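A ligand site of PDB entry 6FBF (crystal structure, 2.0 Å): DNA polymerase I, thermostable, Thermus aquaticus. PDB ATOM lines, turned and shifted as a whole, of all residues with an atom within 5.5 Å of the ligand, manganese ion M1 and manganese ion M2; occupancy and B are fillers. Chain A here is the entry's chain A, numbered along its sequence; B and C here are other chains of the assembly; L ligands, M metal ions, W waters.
Water W2 bridges OE1 of Glu 495 (2.6 Å) and O of Val 492 (3.2 Å). Water W4 bridges O5 of the ligand (2.6 Å) and OP1 of DC 12 of chain B (3.3 Å). Water W3 lies within hydrogen-bond range of O of Asp 319 (3.1 Å) and O7 of the ligand (3.5 Å). Water W5 lies within hydrogen-bond range of NH2 of Arg 369 (2.5 Å), OP2 of DC 12 of chain B (2.7 Å) and O5 of the ligand (3.0 Å). Water W7 lies within hydrogen-bond range of OE2 of Glu 324 (2.8 Å), NE2 of Gln 463 (2.9 Å), ND2 of Asn 459 (2.9 Å) and N3 of the ligand (3.4 Å). Water W6 lies within hydrogen-bond range of NH2 of Arg 282 (2.8 Å), OE2 of Glu 324 (2.8 Å) and O11 of the ligand (3.4 Å).
Ser 321 touches the ligand (CA to O7, 3.6 Å). Phe 376 touches the ligand. CD2 of Tyr 380 touches N2 of the ligand, at 3.5 Å. Hydrophobic or aromatic side chains within 4 Å of the ligand: Ile 323, His 348, Phe 376 and Tyr 380. 17 residues have an atom within 4 Å of the ligand: Arg 282, Asp 319, Tyr 320, Ser 321, Gln 322, Ile 323, Glu 324, His 348, Arg 368, Arg 369, Lys 372, Phe 376, Tyr 380, Asp 494, DC 12 of chain B, DC 4 of chain C and DG 5 of chain C. Along chain A the residues within 4 Å of the ligand span positions 282 to 494. The nearest printed residue that does not touch the ligand is Thr 373 (4.3 Å).
Manganese ion M1 is bound by the side-chain carboxylate of Asp 494 (2.1 Å), the side-chain carboxylate of Asp 319 (2.2 Å), water W2 (2.2 Å), water W4 (2.2 Å), an oxygen (O2) of the ligand (2.2 Å) and O3' of DC 12 of chain B (2.3 Å).
The guanidinium group (NH1) of Arg 368 lies within salt-bridge range of an oxygen (O10) of the ligand (2.4 Å). The side-chain amino group of Lys 372 is in salt-bridge range of an oxygen (O10) of the ligand (2.7 Å). O2 of DC 4 of chain C lies within hydrogen-bond range of N2 of the ligand (2.7 Å). The backbone NH of Ile 323 lies close to an oxygen (O3) of the ligand. The guanidinium group of Arg 369 lies within hydrogen-bond range of an oxygen (O1) of the ligand (2.9 Å). An oxygen (O6) of the ligand is in hydrogen-bond range of a ring nitrogen (NE2) of His 348 (3.0 Å). The guanidinium group of Arg 282 is in hydrogen-bond range of an oxygen (O11) of the ligand, at 3.2 Å. N2 of the ligand sits close to N3 of DG 5 of chain C (3.4 Å). The backbone NH (N) of Glu 324 lies within hydrogen-bond range of an oxygen (O8) of the ligand. An oxygen (O7) of the ligand is in hydrogen-bond range of the backbone NH (N) of Gln 322 (3.3 Å).
O2 of DC 12 of chain B is in hydrogen-bond range of the guanidinium group of Arg 282 (2.9 Å). O2 of DC 12 of chain B sits close to N2 of DG 5 of chain C. NH2 of Arg 368 is in salt-bridge range of OD2 of Asp 346, 3.0 Å away. The side-chain hydroxyl of Thr 373 sits at hydrogen-bond distance from the guanidinium group of Arg 369. The backbone NH (N) of His 348 is in hydrogen-bond range of the side-chain carboxylate (OD1) of Asp 346 (3.0 Å). NH1 of Arg 282 lies within hydrogen-bond range of N2 of DG 5 of chain C (3.5 Å). NE of Arg 282 lies close to OE1 of Gln 463, 3.5 Å away. The side-chain amide nitrogen (NE2) of Gln 322 lies within hydrogen-bond range of the side-chain hydroxyl (OG) of Ser 321 (3.4 Å).
Manganese ion M2 is bound by an oxygen (O3) of the ligand (2.1 Å), the backbone carbonyl oxygen of Tyr 320 (2.1 Å), an oxygen (O4) of the ligand (2.1 Å), the side-chain carboxylate of Asp 319 (2.1 Å), the side-chain carboxylate of Asp 494 (2.1 Å) and an oxygen (O2) of the ligand (2.2 Å). Manganese ion M2 has six donor atoms within binding distance.
The nearest printed residue that does not touch manganese ion M2 is Ser 321 (4.3 Å).
Of the 25 residues printed, 3 come within 4 Å of manganese ion M1.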
ATOM      1  N   ARG A 282      17.255  11.804   8.980  1.00  0.00           N
ATOM      2  CA  ARG A 282      17.743  11.259   7.730  1.00  0.00           C
ATOM      3  C   ARG A 282      17.429  12.197   6.565  1.00  0.00           C
ATOM      4  O   ARG A 282      16.467  12.972   6.606  1.00  0.00           O
ATOM      5  CB  ARG A 282      17.093   9.900   7.438  1.00  0.00           C
ATOM      6  CG  ARG A 282      17.798   8.697   8.029  1.00  0.00           C
ATOM      7  CD  ARG A 282      17.170   7.425   7.461  1.00  0.00           C
ATOM      8  NE  ARG A 282      17.886   6.216   7.826  1.00  0.00           N
ATOM      9  CZ  ARG A 282      17.608   5.012   7.345  1.00  0.00           C
ATOM     10  NH1 ARG A 282      16.642   4.857   6.458  1.00  0.00           N
ATOM     11  NH2 ARG A 282      18.318   3.962   7.744  1.00  0.00           N
ATOM     12  N   ASP A 319      30.478   2.170   2.876  1.00  0.00           N
ATOM     13  CA  ASP A 319      29.267   1.850   3.612  1.00  0.00           C
ATOM     14  C   ASP A 319      29.633   1.435   5.029  1.00  0.00           C
ATOM     15  O   ASP A 319      30.431   0.514   5.222  1.00  0.00           O
ATOM     16  CB  ASP A 319      28.484   0.736   2.915  1.00  0.00           C
ATOM     17  CG  ASP A 319      27.134   0.466   3.568  1.00  0.00           C
ATOM     18  OD1 ASP A 319      27.110   0.128   4.774  1.00  0.00           O
ATOM     19  OD2 ASP A 319      26.101   0.582   2.881  1.00  0.00           O
ATOM     20  N   TYR A 320      29.062   2.115   6.024  1.00  0.00           N
ATOM     21  CA  TYR A 320      29.320   1.774   7.418  1.00  0.00           C
ATOM     22  C   TYR A 320      28.854   0.359   7.712  1.00  0.00           C
ATOM     23  O   TYR A 320      27.801  -0.089   7.227  1.00  0.00           O
ATOM     24  CB  TYR A 320      28.608   2.758   8.350  1.00  0.00           C
ATOM     25  CG  TYR A 320      29.260   4.118   8.458  1.00  0.00           C
ATOM     26  CD1 TYR A 320      30.389   4.300   9.251  1.00  0.00           C
ATOM     27  CD2 TYR A 320      28.739   5.220   7.795  1.00  0.00           C
ATOM     28  CE1 TYR A 320      30.982   5.540   9.364  1.00  0.00           C
ATOM     29  CE2 TYR A 320      29.331   6.460   7.908  1.00  0.00           C
ATOM     30  CZ  TYR A 320      30.448   6.618   8.693  1.00  0.00           C
ATOM     31  OH  TYR A 320      31.041   7.858   8.806  1.00  0.00           O
ATOM     32  N   SER A 321      29.631  -0.349   8.512  1.00  0.00           N
ATOM     33  CA  SER A 321      29.309  -1.716   8.912  1.00  0.00           C
ATOM     34  C   SER A 321      28.398  -1.683  10.145  1.00  0.00           C
ATOM     35  O   SER A 321      28.760  -1.074  11.163  1.00  0.00           O
ATOM     36  CB  SER A 321      30.576  -2.513   9.205  1.00  0.00           C
ATOM     37  OG  SER A 321      30.277  -3.816   9.653  1.00  0.00           O
ATOM     38  N   GLN A 322      27.244  -2.339  10.052  1.00  0.00           N
ATOM     39  CA  GLN A 322      26.357  -2.546  11.194  1.00  0.00           C
ATOM     40  C   GLN A 322      26.119  -1.252  11.960  1.00  0.00           C
ATOM     41  O   GLN A 322      26.202  -1.206  13.193  1.00  0.00           O
ATOM     42  CB  GLN A 322      26.921  -3.631  12.118  1.00  0.00           C
ATOM     43  CG  GLN A 322      27.342  -4.909  11.408  1.00  0.00           C
ATOM     44  CD  GLN A 322      28.052  -5.872  12.335  1.00  0.00           C
ATOM     45  OE1 GLN A 322      27.436  -6.533  13.171  1.00  0.00           O
ATOM     46  NE2 GLN A 322      29.374  -5.957  12.198  1.00  0.00           N
ATOM     47  N   ILE A 323      25.812  -0.190  11.223  1.00  0.00           N
ATOM     48  CA  ILE A 323      25.922   1.159  11.792  1.00  0.00           C
ATOM     49  C   ILE A 323      25.040   1.310  13.027  1.00  0.00           C
ATOM     50  O   ILE A 323      25.515   1.681  14.103  1.00  0.00           O
ATOM     51  CB  ILE A 323      25.620   2.227  10.721  1.00  0.00           C
ATOM     52  CG1 ILE A 323      25.729   3.637  11.309  1.00  0.00           C
ATOM     53  CG2 ILE A 323      24.254   2.024  10.072  1.00  0.00           C
ATOM     54  CD1 ILE A 323      27.105   3.975  11.860  1.00  0.00           C
ATOM     55  N   GLU A 324      23.746   1.015  12.900  1.00  0.00           N
ATOM     56  CA  GLU A 324      22.844   1.290  14.018  1.00  0.00           C
ATOM     57  C   GLU A 324      23.125   0.385  15.210  1.00  0.00           C
ATOM     58  O   GLU A 324      22.893   0.778  16.352  1.00  0.00           O
ATOM     59  CB  GLU A 324      21.380   1.171  13.579  1.00  0.00           C
ATOM     60  CG  GLU A 324      20.878   2.416  12.830  1.00  0.00           C
ATOM     61  CD  GLU A 324      19.362   2.440  12.651  1.00  0.00           C
ATOM     62  OE1 GLU A 324      18.642   1.844  13.482  1.00  0.00           O
ATOM     63  OE2 GLU A 324      18.899   3.048  11.670  1.00  0.00           O
ATOM     64  N   LEU A 325      23.644  -0.821  14.967  1.00  0.00           N
ATOM     65  CA  LEU A 325      24.058  -1.677  16.072  1.00  0.00           C
ATOM     66  C   LEU A 325      25.253  -1.081  16.817  1.00  0.00           C
ATOM     67  O   LEU A 325      25.302  -1.115  18.044  1.00  0.00           O
ATOM     68  CB  LEU A 325      24.383  -3.087  15.570  1.00  0.00           C
ATOM     69  CG  LEU A 325      23.241  -3.849  14.890  1.00  0.00           C
ATOM     70  CD1 LEU A 325      23.672  -5.281  14.587  1.00  0.00           C
ATOM     71  CD2 LEU A 325      21.973  -3.841  15.735  1.00  0.00           C
ATOM     72  N   ASP A 346      30.452  -9.996  13.468  1.00  0.00           N
ATOM     73  CA  ASP A 346      29.429  -9.483  12.568  1.00  0.00           C
ATOM     74  C   ASP A 346      28.096 -10.139  12.923  1.00  0.00           C
ATOM     75  O   ASP A 346      27.878 -11.310  12.624  1.00  0.00           O
ATOM     76  CB  ASP A 346      29.802  -9.748  11.110  1.00  0.00           C
ATOM     77  CG  ASP A 346      28.934  -8.999  10.126  1.00  0.00           C
ATOM     78  OD1 ASP A 346      27.706  -8.971  10.311  1.00  0.00           O
ATOM     79  OD2 ASP A 346      29.487  -8.429   9.161  1.00  0.00           O
ATOM     80  N   HIS A 348      25.110  -9.568  11.754  1.00  0.00           N
ATOM     81  CA  HIS A 348      24.326  -9.927  10.583  1.00  0.00           C
ATOM     82  C   HIS A 348      24.735 -11.287  10.045  1.00  0.00           C
ATOM     83  O   HIS A 348      23.891 -12.108   9.695  1.00  0.00           O
ATOM     84  CB  HIS A 348      24.466  -8.851   9.508  1.00  0.00           C
ATOM     85  CG  HIS A 348      23.872  -7.528   9.900  1.00  0.00           C
ATOM     86  ND1 HIS A 348      22.940  -7.395  10.911  1.00  0.00           N
ATOM     87  CD2 HIS A 348      24.083  -6.283   9.417  1.00  0.00           C
ATOM     88  CE1 HIS A 348      22.607  -6.121  11.026  1.00  0.00           C
ATOM     89  NE2 HIS A 348      23.280  -5.429  10.129  1.00  0.00           N
ATOM     90  N   ARG A 368      22.313 -12.383   4.015  1.00  0.00           N
ATOM     91  CA  ARG A 368      22.649 -11.352   4.983  1.00  0.00           C
ATOM     92  C   ARG A 368      21.557 -10.300   5.072  1.00  0.00           C
ATOM     93  O   ARG A 368      21.224  -9.829   6.168  1.00  0.00           O
ATOM     94  CB  ARG A 368      23.987 -10.713   4.618  1.00  0.00           C
ATOM     95  CG  ARG A 368      24.602  -9.897   5.741  1.00  0.00           C
ATOM     96  CD  ARG A 368      26.118  -9.862   5.637  1.00  0.00           C
ATOM     97  NE  ARG A 368      26.708  -9.078   6.718  1.00  0.00           N
ATOM     98  CZ  ARG A 368      26.662  -7.753   6.769  1.00  0.00           C
ATOM     99  NH1 ARG A 368      26.054  -7.075   5.810  1.00  0.00           N
ATOM    100  NH2 ARG A 368      27.227  -7.111   7.788  1.00  0.00           N
ATOM    101  N   ARG A 369      20.972  -9.911   3.941  1.00  0.00           N
ATOM    102  CA  ARG A 369      19.856  -8.975   3.969  1.00  0.00           C
ATOM    103  C   ARG A 369      18.691  -9.551   4.774  1.00  0.00           C
ATOM    104  O   ARG A 369      18.037  -8.833   5.536  1.00  0.00           O
ATOM    105  CB  ARG A 369      19.412  -8.639   2.538  1.00  0.00           C
ATOM    106  CG  ARG A 369      18.173  -7.759   2.426  1.00  0.00           C
ATOM    107  CD  ARG A 369      18.338  -6.410   3.106  1.00  0.00           C
ATOM    108  NE  ARG A 369      17.665  -6.357   4.403  1.00  0.00           N
ATOM    109  CZ  ARG A 369      17.410  -5.232   5.078  1.00  0.00           C
ATOM    110  NH1 ARG A 369      16.793  -5.299   6.241  1.00  0.00           N
ATOM    111  NH2 ARG A 369      17.781  -4.062   4.590  1.00  0.00           N
ATOM    112  N   LYS A 372      19.430  -9.022   8.365  1.00  0.00           N
ATOM    113  CA  LYS A 372      19.230  -7.640   8.803  1.00  0.00           C
ATOM    114  C   LYS A 372      17.795  -7.407   9.256  1.00  0.00           C
ATOM    115  O   LYS A 372      17.552  -6.800  10.298  1.00  0.00           O
ATOM    116  CB  LYS A 372      19.604  -6.674   7.682  1.00  0.00           C
ATOM    117  CG  LYS A 372      21.086  -6.641   7.357  1.00  0.00           C
ATOM    118  CD  LYS A 372      21.355  -5.691   6.203  1.00  0.00           C
ATOM    119  CE  LYS A 372      22.848  -5.532   5.959  1.00  0.00           C
ATOM    120  NZ  LYS A 372      23.131  -4.608   4.835  1.00  0.00           N
ATOM    121  N   THR A 373      16.833  -7.869   8.459  1.00  0.00           N
ATOM    122  CA  THR A 373      15.432  -7.738   8.839  1.00  0.00           C
ATOM    123  C   THR A 373      15.196  -8.278  10.242  1.00  0.00           C
ATOM    124  O   THR A 373      14.525  -7.638  11.063  1.00  0.00           O
ATOM    125  CB  THR A 373      14.534  -8.466   7.835  1.00  0.00           C
ATOM    126  OG1 THR A 373      14.773  -7.939   6.517  1.00  0.00           O
ATOM    127  CG2 THR A 373      13.057  -8.292   8.179  1.00  0.00           C
ATOM    128  N   PHE A 376      17.297  -6.107  13.143  1.00  0.00           N
ATOM    129  CA  PHE A 376      16.650  -4.827  13.391  1.00  0.00           C
ATOM    130  C   PHE A 376      15.174  -4.983  13.701  1.00  0.00           C
ATOM    131  O   PHE A 376      14.629  -4.229  14.504  1.00  0.00           O
ATOM    132  CB  PHE A 376      16.869  -3.899  12.184  1.00  0.00           C
ATOM    133  CG  PHE A 376      18.311  -3.567  11.926  1.00  0.00           C
ATOM    134  CD1 PHE A 376      19.040  -2.819  12.842  1.00  0.00           C
ATOM    135  CD2 PHE A 376      18.942  -4.011  10.774  1.00  0.00           C
ATOM    136  CE1 PHE A 376      20.378  -2.516  12.613  1.00  0.00           C
ATOM    137  CE2 PHE A 376      20.281  -3.708  10.545  1.00  0.00           C
ATOM    138  CZ  PHE A 376      21.000  -2.964  11.462  1.00  0.00           C
ATOM    139  N   GLY A 377      14.506  -5.959  13.081  1.00  0.00           N
ATOM    140  CA  GLY A 377      13.113  -6.208  13.412  1.00  0.00           C
ATOM    141  C   GLY A 377      12.924  -6.526  14.874  1.00  0.00           C
ATOM    142  O   GLY A 377      12.089  -5.919  15.556  1.00  0.00           O
ATOM    143  N   TYR A 380      13.735  -3.385  17.238  1.00  0.00           N
ATOM    144  CA  TYR A 380      12.739  -2.319  17.259  1.00  0.00           C
ATOM    145  C   TYR A 380      11.312  -2.839  17.455  1.00  0.00           C
ATOM    146  O   TYR A 380      10.359  -2.189  17.016  1.00  0.00           O
ATOM    147  CB  TYR A 380      12.847  -1.485  15.982  1.00  0.00           C
ATOM    148  CG  TYR A 380      14.185  -0.777  15.870  1.00  0.00           C
ATOM    149  CD1 TYR A 380      14.564   0.167  16.805  1.00  0.00           C
ATOM    150  CD2 TYR A 380      15.063  -1.077  14.840  1.00  0.00           C
ATOM    151  CE1 TYR A 380      15.779   0.813  16.724  1.00  0.00           C
ATOM    152  CE2 TYR A 380      16.290  -0.439  14.740  1.00  0.00           C
ATOM    153  CZ  TYR A 380      16.648   0.506  15.682  1.00  0.00           C
ATOM    154  OH  TYR A 380      17.863   1.152  15.601  1.00  0.00           O
ATOM    155  N   ASN A 459      13.421   4.291  18.450  1.00  0.00           N
ATOM    156  CA  ASN A 459      14.165   4.080  17.216  1.00  0.00           C
ATOM    157  C   ASN A 459      14.854   5.357  16.752  1.00  0.00           C
ATOM    158  O   ASN A 459      15.959   5.291  16.194  1.00  0.00           O
ATOM    159  CB  ASN A 459      13.242   3.574  16.109  1.00  0.00           C
ATOM    160  CG  ASN A 459      13.860   3.687  14.726  1.00  0.00           C
ATOM    161  OD1 ASN A 459      13.798   4.735  14.092  1.00  0.00           O
ATOM    162  ND2 ASN A 459      14.479   2.601  14.257  1.00  0.00           N
ATOM    163  N   GLN A 463      18.549   5.585  14.766  1.00  0.00           N
ATOM    164  CA  GLN A 463      18.610   5.968  13.363  1.00  0.00           C
ATOM    165  C   GLN A 463      19.054   7.420  13.198  1.00  0.00           C
ATOM    166  O   GLN A 463      19.772   7.747  12.247  1.00  0.00           O
ATOM    167  CB  GLN A 463      17.238   5.754  12.710  1.00  0.00           C
ATOM    168  CG  GLN A 463      17.180   6.084  11.226  1.00  0.00           C
ATOM    169  CD  GLN A 463      15.796   5.918  10.647  1.00  0.00           C
ATOM    170  OE1 GLN A 463      15.258   6.829  10.011  1.00  0.00           O
ATOM    171  NE2 GLN A 463      15.202   4.742  10.855  1.00  0.00           N
ATOM    172  N   VAL A 492      23.395   7.192   0.656  1.00  0.00           N
ATOM    173  CA  VAL A 492      22.312   6.246   0.931  1.00  0.00           C
ATOM    174  C   VAL A 492      22.287   5.963   2.429  1.00  0.00           C
ATOM    175  O   VAL A 492      22.470   4.826   2.855  1.00  0.00           O
ATOM    176  CB  VAL A 492      22.476   4.958   0.110  1.00  0.00           C
ATOM    177  CG1 VAL A 492      21.142   4.236   0.006  1.00  0.00           C
ATOM    178  CG2 VAL A 492      23.029   5.258  -1.276  1.00  0.00           C
ATOM    179  N   ASP A 494      23.796   5.485   5.139  1.00  0.00           N
ATOM    180  CA  ASP A 494      25.079   5.164   5.764  1.00  0.00           C
ATOM    181  C   ASP A 494      26.136   4.846   4.705  1.00  0.00           C
ATOM    182  O   ASP A 494      27.155   4.214   5.029  1.00  0.00           O
ATOM    183  CB  ASP A 494      24.933   3.999   6.740  1.00  0.00           C
ATOM    184  CG  ASP A 494      24.865   2.649   6.054  1.00  0.00           C
ATOM    185  OD1 ASP A 494      24.397   2.584   4.895  1.00  0.00           O
ATOM    186  OD2 ASP A 494      25.276   1.650   6.685  1.00  0.00           O
ATOM    187  N   GLU A 495      25.920   5.287   3.474  1.00  0.00           N
ATOM    188  CA  GLU A 495      26.786   4.940   2.355  1.00  0.00           C
ATOM    189  C   GLU A 495      27.035   6.183   1.512  1.00  0.00           C
ATOM    190  O   GLU A 495      26.177   7.065   1.412  1.00  0.00           O
ATOM    191  CB  GLU A 495      26.167   3.833   1.495  1.00  0.00           C
ATOM    192  CG  GLU A 495      26.924   3.520   0.195  1.00  0.00           C
ATOM    193  CD  GLU A 495      26.166   2.557  -0.702  1.00  0.00           C
ATOM    194  OE1 GLU A 495      25.061   2.121  -0.320  1.00  0.00           O
ATOM    195  OE2 GLU A 495      26.689   2.234  -1.795  1.00  0.00           O
ATOM    196  P    DC B  12      20.360  -1.227   0.193  1.00  0.00           P
ATOM    197  OP1  DC B  12      21.704  -0.967  -0.348  1.00  0.00           O
ATOM    198  OP2  DC B  12      19.998  -2.589   0.642  1.00  0.00           O
ATOM    199  O5'  DC B  12      20.089  -0.237   1.409  1.00  0.00           O
ATOM    200  C5'  DC B  12      20.485   1.134   1.311  1.00  0.00           C
ATOM    201  C4'  DC B  12      20.162   1.894   2.580  1.00  0.00           C
ATOM    202  O4'  DC B  12      18.729   1.986   2.721  1.00  0.00           O
ATOM    203  C3'  DC B  12      20.650   1.250   3.859  1.00  0.00           C
ATOM    204  O3'  DC B  12      21.977   1.665   4.151  1.00  0.00           O
ATOM    205  C2'  DC B  12      19.654   1.733   4.900  1.00  0.00           C
ATOM    206  C1'  DC B  12      18.371   1.954   4.098  1.00  0.00           C
ATOM    207  N1   DC B  12      17.346   0.899   4.301  1.00  0.00           N
ATOM    208  C2   DC B  12      16.440   1.007   5.350  1.00  0.00           C
ATOM    209  O2   DC B  12      16.511   1.992   6.100  1.00  0.00           O
ATOM    210  N3   DC B  12      15.507   0.039   5.521  1.00  0.00           N
ATOM    211  C4   DC B  12      15.469  -0.995   4.691  1.00  0.00           C
ATOM    212  N4   DC B  12      14.528  -1.934   4.890  1.00  0.00           N
ATOM    213  C5   DC B  12      16.382  -1.128   3.605  1.00  0.00           C
ATOM    214  C6   DC B  12      17.296  -0.164   3.449  1.00  0.00           C
ATOM    215  P    DC C   4       5.240  -6.269  13.833  1.00  0.00           P
ATOM    216  OP1  DC C   4       4.792  -6.423  12.428  1.00  0.00           O
ATOM    217  OP2  DC C   4       5.252  -7.443  14.732  1.00  0.00           O
ATOM    218  O5'  DC C   4       6.711  -5.645  13.835  1.00  0.00           O
ATOM    219  C5'  DC C   4       6.931  -4.362  13.275  1.00  0.00           C
ATOM    220  C4'  DC C   4       8.064  -3.653  13.978  1.00  0.00           C
ATOM    221  O4'  DC C   4       9.284  -4.403  13.801  1.00  0.00           O
ATOM    222  C3'  DC C   4       8.360  -2.251  13.465  1.00  0.00           C
ATOM    223  O3'  DC C   4       7.593  -1.275  14.156  1.00  0.00           O
ATOM    224  C2'  DC C   4       9.853  -2.115  13.730  1.00  0.00           C
ATOM    225  C1'  DC C   4      10.364  -3.530  13.526  1.00  0.00           C
ATOM    226  N1   DC C   4      10.853  -3.796  12.136  1.00  0.00           N
ATOM    227  C2   DC C   4      12.055  -3.208  11.718  1.00  0.00           C
ATOM    228  O2   DC C   4      12.685  -2.497  12.496  1.00  0.00           O
ATOM    229  N3   DC C   4      12.487  -3.461  10.456  1.00  0.00           N
ATOM    230  C4   DC C   4      11.780  -4.234   9.636  1.00  0.00           C
ATOM    231  N4   DC C   4      12.262  -4.440   8.405  1.00  0.00           N
ATOM    232  C5   DC C   4      10.553  -4.842  10.052  1.00  0.00           C
ATOM    233  C6   DC C   4      10.130  -4.589  11.300  1.00  0.00           C
ATOM    234  P    DG C   5       6.886  -0.075  13.345  1.00  0.00           P
ATOM    235  OP1  DG C   5       5.914   0.555  14.253  1.00  0.00           O
ATOM    236  OP2  DG C   5       6.443  -0.614  12.039  1.00  0.00           O
ATOM    237  O5'  DG C   5       8.080   0.945  13.072  1.00  0.00           O
ATOM    238  C5'  DG C   5       8.713   1.596  14.155  1.00  0.00           C
ATOM    239  C4'  DG C   5       9.986   2.296  13.713  1.00  0.00           C
ATOM    240  O4'  DG C   5      10.947   1.308  13.256  1.00  0.00           O
ATOM    241  C3'  DG C   5       9.821   3.241  12.540  1.00  0.00           C
ATOM    242  O3'  DG C   5       9.379   4.521  12.968  1.00  0.00           O
ATOM    243  C2'  DG C   5      11.223   3.267  11.959  1.00  0.00           C
ATOM    244  C1'  DG C   5      11.730   1.850  12.206  1.00  0.00           C
ATOM    245  N9   DG C   5      11.630   0.983  11.037  1.00  0.00           N
ATOM    246  C8   DG C   5      10.688   0.010  10.805  1.00  0.00           C
ATOM    247  N7   DG C   5      10.857  -0.601   9.667  1.00  0.00           N
ATOM    248  C5   DG C   5      11.975  -0.002   9.120  1.00  0.00           C
ATOM    249  C6   DG C   5      12.634  -0.242   7.886  1.00  0.00           C
ATOM    250  O6   DG C   5      12.360  -1.080   7.017  1.00  0.00           O
ATOM    251  N1   DG C   5      13.737   0.601   7.717  1.00  0.00           N
ATOM    252  C2   DG C   5      14.138   1.560   8.618  1.00  0.00           C
ATOM    253  N2   DG C   5      15.220   2.279   8.278  1.00  0.00           N
ATOM    254  N3   DG C   5      13.527   1.796   9.765  1.00  0.00           N
ATOM    255  C4   DG C   5      12.457   0.980   9.949  1.00  0.00           C
HETATM  256  N1  LIG L   1      14.818  -2.258   9.553  1.00  0.00           N
HETATM  257  C1  LIG L   1      15.277  -1.230  10.331  1.00  0.00           C
HETATM  258  N2  LIG L   1      14.566  -0.929  11.414  1.00  0.00           N
HETATM  259  N3  LIG L   1      16.380  -0.525  10.048  1.00  0.00           N
HETATM  260  C2  LIG L   1      16.976  -0.932   8.914  1.00  0.00           C
HETATM  261  C3  LIG L   1      16.590  -1.942   8.064  1.00  0.00           C
HETATM  262  C4  LIG L   1      15.414  -2.697   8.392  1.00  0.00           C
HETATM  263  O1  LIG L   1      14.952  -3.648   7.768  1.00  0.00           O
HETATM  264  N4  LIG L   1      17.477  -2.032   6.996  1.00  0.00           N
HETATM  265  C5  LIG L   1      18.372  -1.103   7.233  1.00  0.00           C
HETATM  266  N5  LIG L   1      18.127  -0.407   8.389  1.00  0.00           N
HETATM  267  P1  LIG L   1      22.601  -1.220   5.768  1.00  0.00           P
HETATM  268  P2  LIG L   1      24.116  -2.272   8.079  1.00  0.00           P
HETATM  269  P3  LIG L   1      26.237  -3.758   6.743  1.00  0.00           P
HETATM  270  C6  LIG L   1      18.977   0.607   9.029  1.00  0.00           C
HETATM  271  O2  LIG L   1      23.918  -0.416   5.421  1.00  0.00           O
HETATM  272  O3  LIG L   1      24.853  -1.012   8.099  1.00  0.00           O
HETATM  273  O4  LIG L   1      26.522  -2.388   6.114  1.00  0.00           O
HETATM  274  C7  LIG L   1      19.906   0.023  10.096  1.00  0.00           C
HETATM  275  O5  LIG L   1      22.127  -1.873   4.554  1.00  0.00           O
HETATM  276  O6  LIG L   1      23.452  -2.477   9.489  1.00  0.00           O
HETATM  277  O7  LIG L   1      27.419  -4.346   7.431  1.00  0.00           O
HETATM  278  C8  LIG L   1      21.214  -0.163   9.348  1.00  0.00           C
HETATM  279  O8  LIG L   1      22.312  -0.116  10.246  1.00  0.00           O
HETATM  280  N6  LIG L   1      22.951  -2.299   6.946  1.00  0.00           N
HETATM  281  O9  LIG L   1      25.063  -3.526   7.797  1.00  0.00           O
HETATM  282  O10 LIG L   1      25.657  -4.674   5.665  1.00  0.00           O
HETATM  283  C9  LIG L   1      21.201   1.028   8.399  1.00  0.00           C
HETATM  284  O11 LIG L   1      19.815   1.188   8.026  1.00  0.00           O
HETATM  285  C10 LIG L   1      22.053   0.899   7.172  1.00  0.00           C
HETATM  286  O12 LIG L   1      21.581  -0.206   6.372  1.00  0.00           O
HETATM  287 MN    MN M   1      24.097   0.880   3.632  1.00  0.00          MN
HETATM  288 MN    MN M   2      25.906  -0.386   6.452  1.00  0.00          MN
HETATM  289  O   HOH W   1      25.449  -2.730   3.342  1.00  0.00           O
HETATM  290  O   HOH W   2      23.689   2.075   1.860  1.00  0.00           O
HETATM  291  O   HOH W   3      29.069  -2.226   5.189  1.00  0.00           O
HETATM  292  O   HOH W   4      23.383  -0.851   2.461  1.00  0.00           O
HETATM  293  O   HOH W   5      19.812  -3.234   3.307  1.00  0.00           O
HETATM  294  O   HOH W   6      20.422   4.187   9.575  1.00  0.00           O
HETATM  295  O   HOH W   7      16.234   2.282  11.931  1.00  0.00           O
